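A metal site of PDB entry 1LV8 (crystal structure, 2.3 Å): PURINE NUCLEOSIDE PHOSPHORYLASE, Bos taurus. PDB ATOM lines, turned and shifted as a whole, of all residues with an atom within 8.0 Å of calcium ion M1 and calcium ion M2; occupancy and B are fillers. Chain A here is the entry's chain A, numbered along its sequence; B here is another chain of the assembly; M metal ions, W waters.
Along chain A the residues within 4 Å of calcium ion M1 span positions 51 to 58. The nearest printed residue that does not touch calcium ion M1 is Ser 51 of chain B (4.4 Å).
Of the 21 residues printed, 3 come within 4 Å of calcium ion M2.
Calcium ion M1 is bound by water W3 (2.0 Å), the side-chain carboxylate (OE2) of Glu 58 of chain A (2.2 Å), the side-chain carboxylate (OE1) of Glu 58 of chain B (2.4 Å), the backbone carbonyl oxygen (O) of Ser 51 of chain A (2.4 Å), the side-chain carboxylate (OE2) of Glu 58 of chain B (2.5 Å), water W4 (2.5 Å) and water W5 (2.7 Å). Calcium ion M1 has seven donor atoms within binding distance.
Calcium ion M2 is bound by OE2 of Glu 58 of chain B (2.1 Å), O of Ser 51 of chain B (2.3 Å), OE2 of Glu 58 of chain A (2.3 Å), water W2 (2.4 Å), OE1 of Glu 58 of chain A (2.4 Å), water W1 (2.5 Å) and water W6 (2.5 Å). Calcium ion M2 has seven donor atoms within binding distance.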
ATOM      1  N   ASP A  49      20.569   5.836  -4.340  1.00  0.00           N
ATOM      2  CA  ASP A  49      19.316   6.583  -4.306  1.00  0.00           C
ATOM      3  C   ASP A  49      19.318   7.321  -2.976  1.00  0.00           C
ATOM      4  O   ASP A  49      19.860   6.807  -1.994  1.00  0.00           O
ATOM      5  CB  ASP A  49      18.121   5.661  -4.361  1.00  0.00           C
ATOM      6  CG  ASP A  49      17.929   5.087  -5.740  1.00  0.00           C
ATOM      7  OD1 ASP A  49      18.080   5.848  -6.720  1.00  0.00           O
ATOM      8  OD2 ASP A  49      17.625   3.882  -5.828  1.00  0.00           O
ATOM      9  N   TYR A  50      18.774   8.533  -2.956  1.00  0.00           N
ATOM     10  CA  TYR A  50      18.750   9.293  -1.700  1.00  0.00           C
ATOM     11  C   TYR A  50      18.042   8.432  -0.677  1.00  0.00           C
ATOM     12  O   TYR A  50      18.495   8.311   0.448  1.00  0.00           O
ATOM     13  CB  TYR A  50      17.950  10.585  -1.838  1.00  0.00           C
ATOM     14  CG  TYR A  50      18.615  11.619  -2.694  1.00  0.00           C
ATOM     15  CD1 TYR A  50      19.995  11.612  -2.895  1.00  0.00           C
ATOM     16  CD2 TYR A  50      17.873  12.634  -3.249  1.00  0.00           C
ATOM     17  CE1 TYR A  50      20.611  12.600  -3.654  1.00  0.00           C
ATOM     18  CE2 TYR A  50      18.467  13.624  -3.978  1.00  0.00           C
ATOM     19  CZ  TYR A  50      19.829  13.605  -4.188  1.00  0.00           C
ATOM     20  OH  TYR A  50      20.356  14.621  -4.930  1.00  0.00           O
ATOM     21  N   SER A  51      16.913   7.857  -1.098  1.00  0.00           N
ATOM     22  CA  SER A  51      16.096   7.035  -0.238  1.00  0.00           C
ATOM     23  C   SER A  51      16.843   5.959   0.530  1.00  0.00           C
ATOM     24  O   SER A  51      16.387   5.544   1.587  1.00  0.00           O
ATOM     25  CB  SER A  51      14.963   6.404  -1.052  1.00  0.00           C
ATOM     26  OG  SER A  51      15.461   5.416  -1.965  1.00  0.00           O
ATOM     27  N   GLU A  52      17.981   5.511   0.024  1.00  0.00           N
ATOM     28  CA  GLU A  52      18.704   4.432   0.737  1.00  0.00           C
ATOM     29  C   GLU A  52      19.842   4.887   1.644  1.00  0.00           C
ATOM     30  O   GLU A  52      20.325   4.115   2.482  1.00  0.00           O
ATOM     31  CB  GLU A  52      19.265   3.391  -0.247  1.00  0.00           C
ATOM     32  CG  GLU A  52      20.558   3.800  -0.934  1.00  0.00           C
ATOM     33  CD  GLU A  52      21.072   2.745  -1.908  1.00  0.00           C
ATOM     34  OE1 GLU A  52      21.085   3.002  -3.142  1.00  0.00           O
ATOM     35  OE2 GLU A  52      21.443   1.661  -1.434  1.00  0.00           O
ATOM     36  N   ILE A  53      20.268   6.129   1.485  1.00  0.00           N
ATOM     37  CA  ILE A  53      21.358   6.633   2.329  1.00  0.00           C
ATOM     38  C   ILE A  53      20.865   7.045   3.709  1.00  0.00           C
ATOM     39  O   ILE A  53      19.979   7.858   3.837  1.00  0.00           O
ATOM     40  CB  ILE A  53      22.034   7.853   1.671  1.00  0.00           C
ATOM     41  CG1 ILE A  53      22.400   7.509   0.217  1.00  0.00           C
ATOM     42  CG2 ILE A  53      23.262   8.230   2.482  1.00  0.00           C
ATOM     43  CD1 ILE A  53      22.793   8.668  -0.618  1.00  0.00           C
ATOM     44  N   PRO A  54      21.476   6.489   4.755  1.00  0.00           N
ATOM     45  CA  PRO A  54      21.065   6.829   6.122  1.00  0.00           C
ATOM     46  C   PRO A  54      20.981   8.344   6.304  1.00  0.00           C
ATOM     47  O   PRO A  54      21.864   9.062   5.833  1.00  0.00           O
ATOM     48  CB  PRO A  54      22.188   6.244   6.978  1.00  0.00           C
ATOM     49  CG  PRO A  54      22.706   5.124   6.155  1.00  0.00           C
ATOM     50  CD  PRO A  54      22.701   5.686   4.754  1.00  0.00           C
ATOM     51  N   ASN A  55      19.925   8.795   6.970  1.00  0.00           N
ATOM     52  CA  ASN A  55      19.650  10.195   7.298  1.00  0.00           C
ATOM     53  C   ASN A  55      19.375  11.106   6.149  1.00  0.00           C
ATOM     54  O   ASN A  55      19.017  12.266   6.350  1.00  0.00           O
ATOM     55  CB  ASN A  55      20.788  10.795   8.123  1.00  0.00           C
ATOM     56  CG  ASN A  55      21.139   9.927   9.339  1.00  0.00           C
ATOM     57  OD1 ASN A  55      20.273   9.447  10.034  1.00  0.00           O
ATOM     58  ND2 ASN A  55      22.432   9.740   9.579  1.00  0.00           N
ATOM     59  N   PHE A  56      19.498  10.618   4.924  1.00  0.00           N
ATOM     60  CA  PHE A  56      19.242  11.489   3.798  1.00  0.00           C
ATOM     61  C   PHE A  56      17.764  11.878   3.624  1.00  0.00           C
ATOM     62  O   PHE A  56      16.866  11.073   3.784  1.00  0.00           O
ATOM     63  CB  PHE A  56      19.747  10.818   2.499  1.00  0.00           C
ATOM     64  CG  PHE A  56      20.740  11.628   1.710  1.00  0.00           C
ATOM     65  CD1 PHE A  56      22.081  11.674   2.085  1.00  0.00           C
ATOM     66  CD2 PHE A  56      20.346  12.325   0.571  1.00  0.00           C
ATOM     67  CE1 PHE A  56      23.025  12.389   1.353  1.00  0.00           C
ATOM     68  CE2 PHE A  56      21.275  13.045  -0.181  1.00  0.00           C
ATOM     69  CZ  PHE A  56      22.620  13.073   0.207  1.00  0.00           C
ATOM     70  N   PRO A  57      17.503  13.130   3.274  1.00  0.00           N
ATOM     71  CA  PRO A  57      16.104  13.491   3.079  1.00  0.00           C
ATOM     72  C   PRO A  57      15.646  12.787   1.784  1.00  0.00           C
ATOM     73  O   PRO A  57      16.491  12.480   0.912  1.00  0.00           O
ATOM     74  CB  PRO A  57      16.185  15.012   2.857  1.00  0.00           C
ATOM     75  CG  PRO A  57      17.435  15.404   3.549  1.00  0.00           C
ATOM     76  CD  PRO A  57      18.383  14.298   3.171  1.00  0.00           C
ATOM     77  N   GLU A  58      14.341  12.544   1.617  1.00  0.00           N
ATOM     78  CA  GLU A  58      13.881  11.904   0.402  1.00  0.00           C
ATOM     79  C   GLU A  58      13.092  12.861  -0.456  1.00  0.00           C
ATOM     80  O   GLU A  58      12.351  13.701   0.051  1.00  0.00           O
ATOM     81  CB  GLU A  58      13.037  10.666   0.719  1.00  0.00           C
ATOM     82  CG  GLU A  58      13.900   9.486   1.099  1.00  0.00           C
ATOM     83  CD  GLU A  58      13.132   8.216   1.463  1.00  0.00           C
ATOM     84  OE1 GLU A  58      12.069   7.949   0.846  1.00  0.00           O
ATOM     85  OE2 GLU A  58      13.631   7.475   2.358  1.00  0.00           O
ATOM     86  N   SER A  59      13.296  12.745  -1.754  1.00  0.00           N
ATOM     87  CA  SER A  59      12.627  13.601  -2.707  1.00  0.00           C
ATOM     88  C   SER A  59      11.142  13.590  -2.396  1.00  0.00           C
ATOM     89  O   SER A  59      10.663  12.712  -1.665  1.00  0.00           O
ATOM     90  CB  SER A  59      12.913  13.109  -4.125  1.00  0.00           C
ATOM     91  OG  SER A  59      14.318  13.083  -4.342  1.00  0.00           O
ATOM     92  N   ASP B  49      13.329  -2.672  -2.000  1.00  0.00           N
ATOM     93  CA  ASP B  49      13.856  -2.311  -0.686  1.00  0.00           C
ATOM     94  C   ASP B  49      12.827  -1.447   0.040  1.00  0.00           C
ATOM     95  O   ASP B  49      12.238  -0.530  -0.552  1.00  0.00           O
ATOM     96  CB  ASP B  49      15.175  -1.555  -0.844  1.00  0.00           C
ATOM     97  CG  ASP B  49      16.329  -2.454  -1.240  1.00  0.00           C
ATOM     98  OD1 ASP B  49      16.441  -3.555  -0.673  1.00  0.00           O
ATOM     99  OD2 ASP B  49      17.122  -2.054  -2.114  1.00  0.00           O
ATOM    100  N   TYR B  50      12.596  -1.721   1.312  1.00  0.00           N
ATOM    101  CA  TYR B  50      11.623  -0.929   2.069  1.00  0.00           C
ATOM    102  C   TYR B  50      11.828   0.553   1.848  1.00  0.00           C
ATOM    103  O   TYR B  50      10.886   1.275   1.542  1.00  0.00           O
ATOM    104  CB  TYR B  50      11.750  -1.168   3.572  1.00  0.00           C
ATOM    105  CG  TYR B  50      11.287  -2.506   4.021  1.00  0.00           C
ATOM    106  CD1 TYR B  50      10.463  -3.280   3.198  1.00  0.00           C
ATOM    107  CD2 TYR B  50      11.625  -2.994   5.284  1.00  0.00           C
ATOM    108  CE1 TYR B  50       9.980  -4.535   3.631  1.00  0.00           C
ATOM    109  CE2 TYR B  50      11.149  -4.244   5.728  1.00  0.00           C
ATOM    110  CZ  TYR B  50      10.324  -5.007   4.883  1.00  0.00           C
ATOM    111  OH  TYR B  50       9.819  -6.223   5.269  1.00  0.00           O
ATOM    112  N   SER B  51      13.073   0.994   1.967  1.00  0.00           N
ATOM    113  CA  SER B  51      13.445   2.399   1.824  1.00  0.00           C
ATOM    114  C   SER B  51      13.032   3.145   0.541  1.00  0.00           C
ATOM    115  O   SER B  51      12.877   4.366   0.576  1.00  0.00           O
ATOM    116  CB  SER B  51      14.957   2.534   2.041  1.00  0.00           C
ATOM    117  OG  SER B  51      15.677   1.774   1.074  1.00  0.00           O
ATOM    118  N   GLU B  52      12.837   2.442  -0.564  1.00  0.00           N
ATOM    119  CA  GLU B  52      12.457   3.129  -1.807  1.00  0.00           C
ATOM    120  C   GLU B  52      10.953   3.188  -2.025  1.00  0.00           C
ATOM    121  O   GLU B  52      10.475   3.916  -2.892  1.00  0.00           O
ATOM    122  CB  GLU B  52      13.111   2.438  -3.024  1.00  0.00           C
ATOM    123  CG  GLU B  52      12.697   0.978  -3.197  1.00  0.00           C
ATOM    124  CD  GLU B  52      13.323   0.290  -4.424  1.00  0.00           C
ATOM    125  OE1 GLU B  52      13.711  -0.902  -4.298  1.00  0.00           O
ATOM    126  OE2 GLU B  52      13.405   0.914  -5.514  1.00  0.00           O
ATOM    127  N   ILE B  53      10.198   2.408  -1.242  1.00  0.00           N
ATOM    128  CA  ILE B  53       8.757   2.367  -1.394  1.00  0.00           C
ATOM    129  C   ILE B  53       8.071   3.508  -0.660  1.00  0.00           C
ATOM    130  O   ILE B  53       8.186   3.653   0.555  1.00  0.00           O
ATOM    131  CB  ILE B  53       8.173   1.047  -0.902  1.00  0.00           C
ATOM    132  CG1 ILE B  53       8.840  -0.126  -1.618  1.00  0.00           C
ATOM    133  CG2 ILE B  53       6.687   1.032  -1.188  1.00  0.00           C
ATOM    134  CD1 ILE B  53       8.410  -1.491  -1.062  1.00  0.00           C
ATOM    135  N   PRO B  54       7.293   4.317  -1.379  1.00  0.00           N
ATOM    136  CA  PRO B  54       6.636   5.428  -0.678  1.00  0.00           C
ATOM    137  C   PRO B  54       5.937   5.025   0.620  1.00  0.00           C
ATOM    138  O   PRO B  54       5.349   3.941   0.731  1.00  0.00           O
ATOM    139  CB  PRO B  54       5.686   6.012  -1.753  1.00  0.00           C
ATOM    140  CG  PRO B  54       6.469   5.761  -3.066  1.00  0.00           C
ATOM    141  CD  PRO B  54       6.987   4.328  -2.828  1.00  0.00           C
ATOM    142  N   ASN B  55       6.067   5.912   1.596  1.00  0.00           N
ATOM    143  CA  ASN B  55       5.483   5.853   2.928  1.00  0.00           C
ATOM    144  C   ASN B  55       5.887   4.695   3.799  1.00  0.00           C
ATOM    145  O   ASN B  55       5.483   4.635   4.954  1.00  0.00           O
ATOM    146  CB  ASN B  55       3.957   5.917   2.802  1.00  0.00           C
ATOM    147  CG  ASN B  55       3.511   7.108   1.998  1.00  0.00           C
ATOM    148  OD1 ASN B  55       3.916   8.235   2.262  1.00  0.00           O
ATOM    149  ND2 ASN B  55       2.661   6.870   0.999  1.00  0.00           N
ATOM    150  N   PHE B  56       6.642   3.754   3.256  1.00  0.00           N
ATOM    151  CA  PHE B  56       7.080   2.612   4.035  1.00  0.00           C
ATOM    152  C   PHE B  56       8.091   3.024   5.078  1.00  0.00           C
ATOM    153  O   PHE B  56       8.931   3.870   4.820  1.00  0.00           O
ATOM    154  CB  PHE B  56       7.804   1.581   3.167  1.00  0.00           C
ATOM    155  CG  PHE B  56       7.123   0.235   3.113  1.00  0.00           C
ATOM    156  CD1 PHE B  56       5.948   0.084   2.392  1.00  0.00           C
ATOM    157  CD2 PHE B  56       7.683  -0.874   3.737  1.00  0.00           C
ATOM    158  CE1 PHE B  56       5.349  -1.147   2.289  1.00  0.00           C
ATOM    159  CE2 PHE B  56       7.083  -2.119   3.632  1.00  0.00           C
ATOM    160  CZ  PHE B  56       5.907  -2.245   2.892  1.00  0.00           C
ATOM    161  N   PRO B  57       7.995   2.437   6.277  1.00  0.00           N
ATOM    162  CA  PRO B  57       8.907   2.711   7.382  1.00  0.00           C
ATOM    163  C   PRO B  57      10.203   2.085   6.926  1.00  0.00           C
ATOM    164  O   PRO B  57      10.192   1.176   6.090  1.00  0.00           O
ATOM    165  CB  PRO B  57       8.311   1.912   8.556  1.00  0.00           C
ATOM    166  CG  PRO B  57       6.803   1.985   8.263  1.00  0.00           C
ATOM    167  CD  PRO B  57       6.773   1.742   6.749  1.00  0.00           C
ATOM    168  N   GLU B  58      11.317   2.542   7.480  1.00  0.00           N
ATOM    169  CA  GLU B  58      12.624   2.009   7.138  1.00  0.00           C
ATOM    170  C   GLU B  58      13.227   1.377   8.366  1.00  0.00           C
ATOM    171  O   GLU B  58      13.090   1.910   9.463  1.00  0.00           O
ATOM    172  CB  GLU B  58      13.530   3.124   6.584  1.00  0.00           C
ATOM    173  CG  GLU B  58      12.908   3.834   5.370  1.00  0.00           C
ATOM    174  CD  GLU B  58      13.858   4.699   4.567  1.00  0.00           C
ATOM    175  OE1 GLU B  58      15.030   4.852   4.967  1.00  0.00           O
ATOM    176  OE2 GLU B  58      13.409   5.217   3.506  1.00  0.00           O
HETATM  177 CA    CA M   1      15.365   6.709   3.484  1.00  0.00          CA
HETATM  178 CA    CA M   2      11.970   5.858   2.084  1.00  0.00          CA
HETATM  179  O   HOH W   1      10.594   3.921   2.755  1.00  0.00           O
HETATM  180  O   HOH W   2       9.891   5.924   0.905  1.00  0.00           O
HETATM  181  O   HOH W   3      17.241   6.485   4.262  1.00  0.00           O
HETATM  182  O   HOH W   4      14.295   8.247   5.193  1.00  0.00           O
HETATM  183  O   HOH W   5      17.017   8.767   2.815  1.00  0.00           O
HETATM  184  O   HOH W   6      10.717   7.027   3.912  1.00  0.00           O
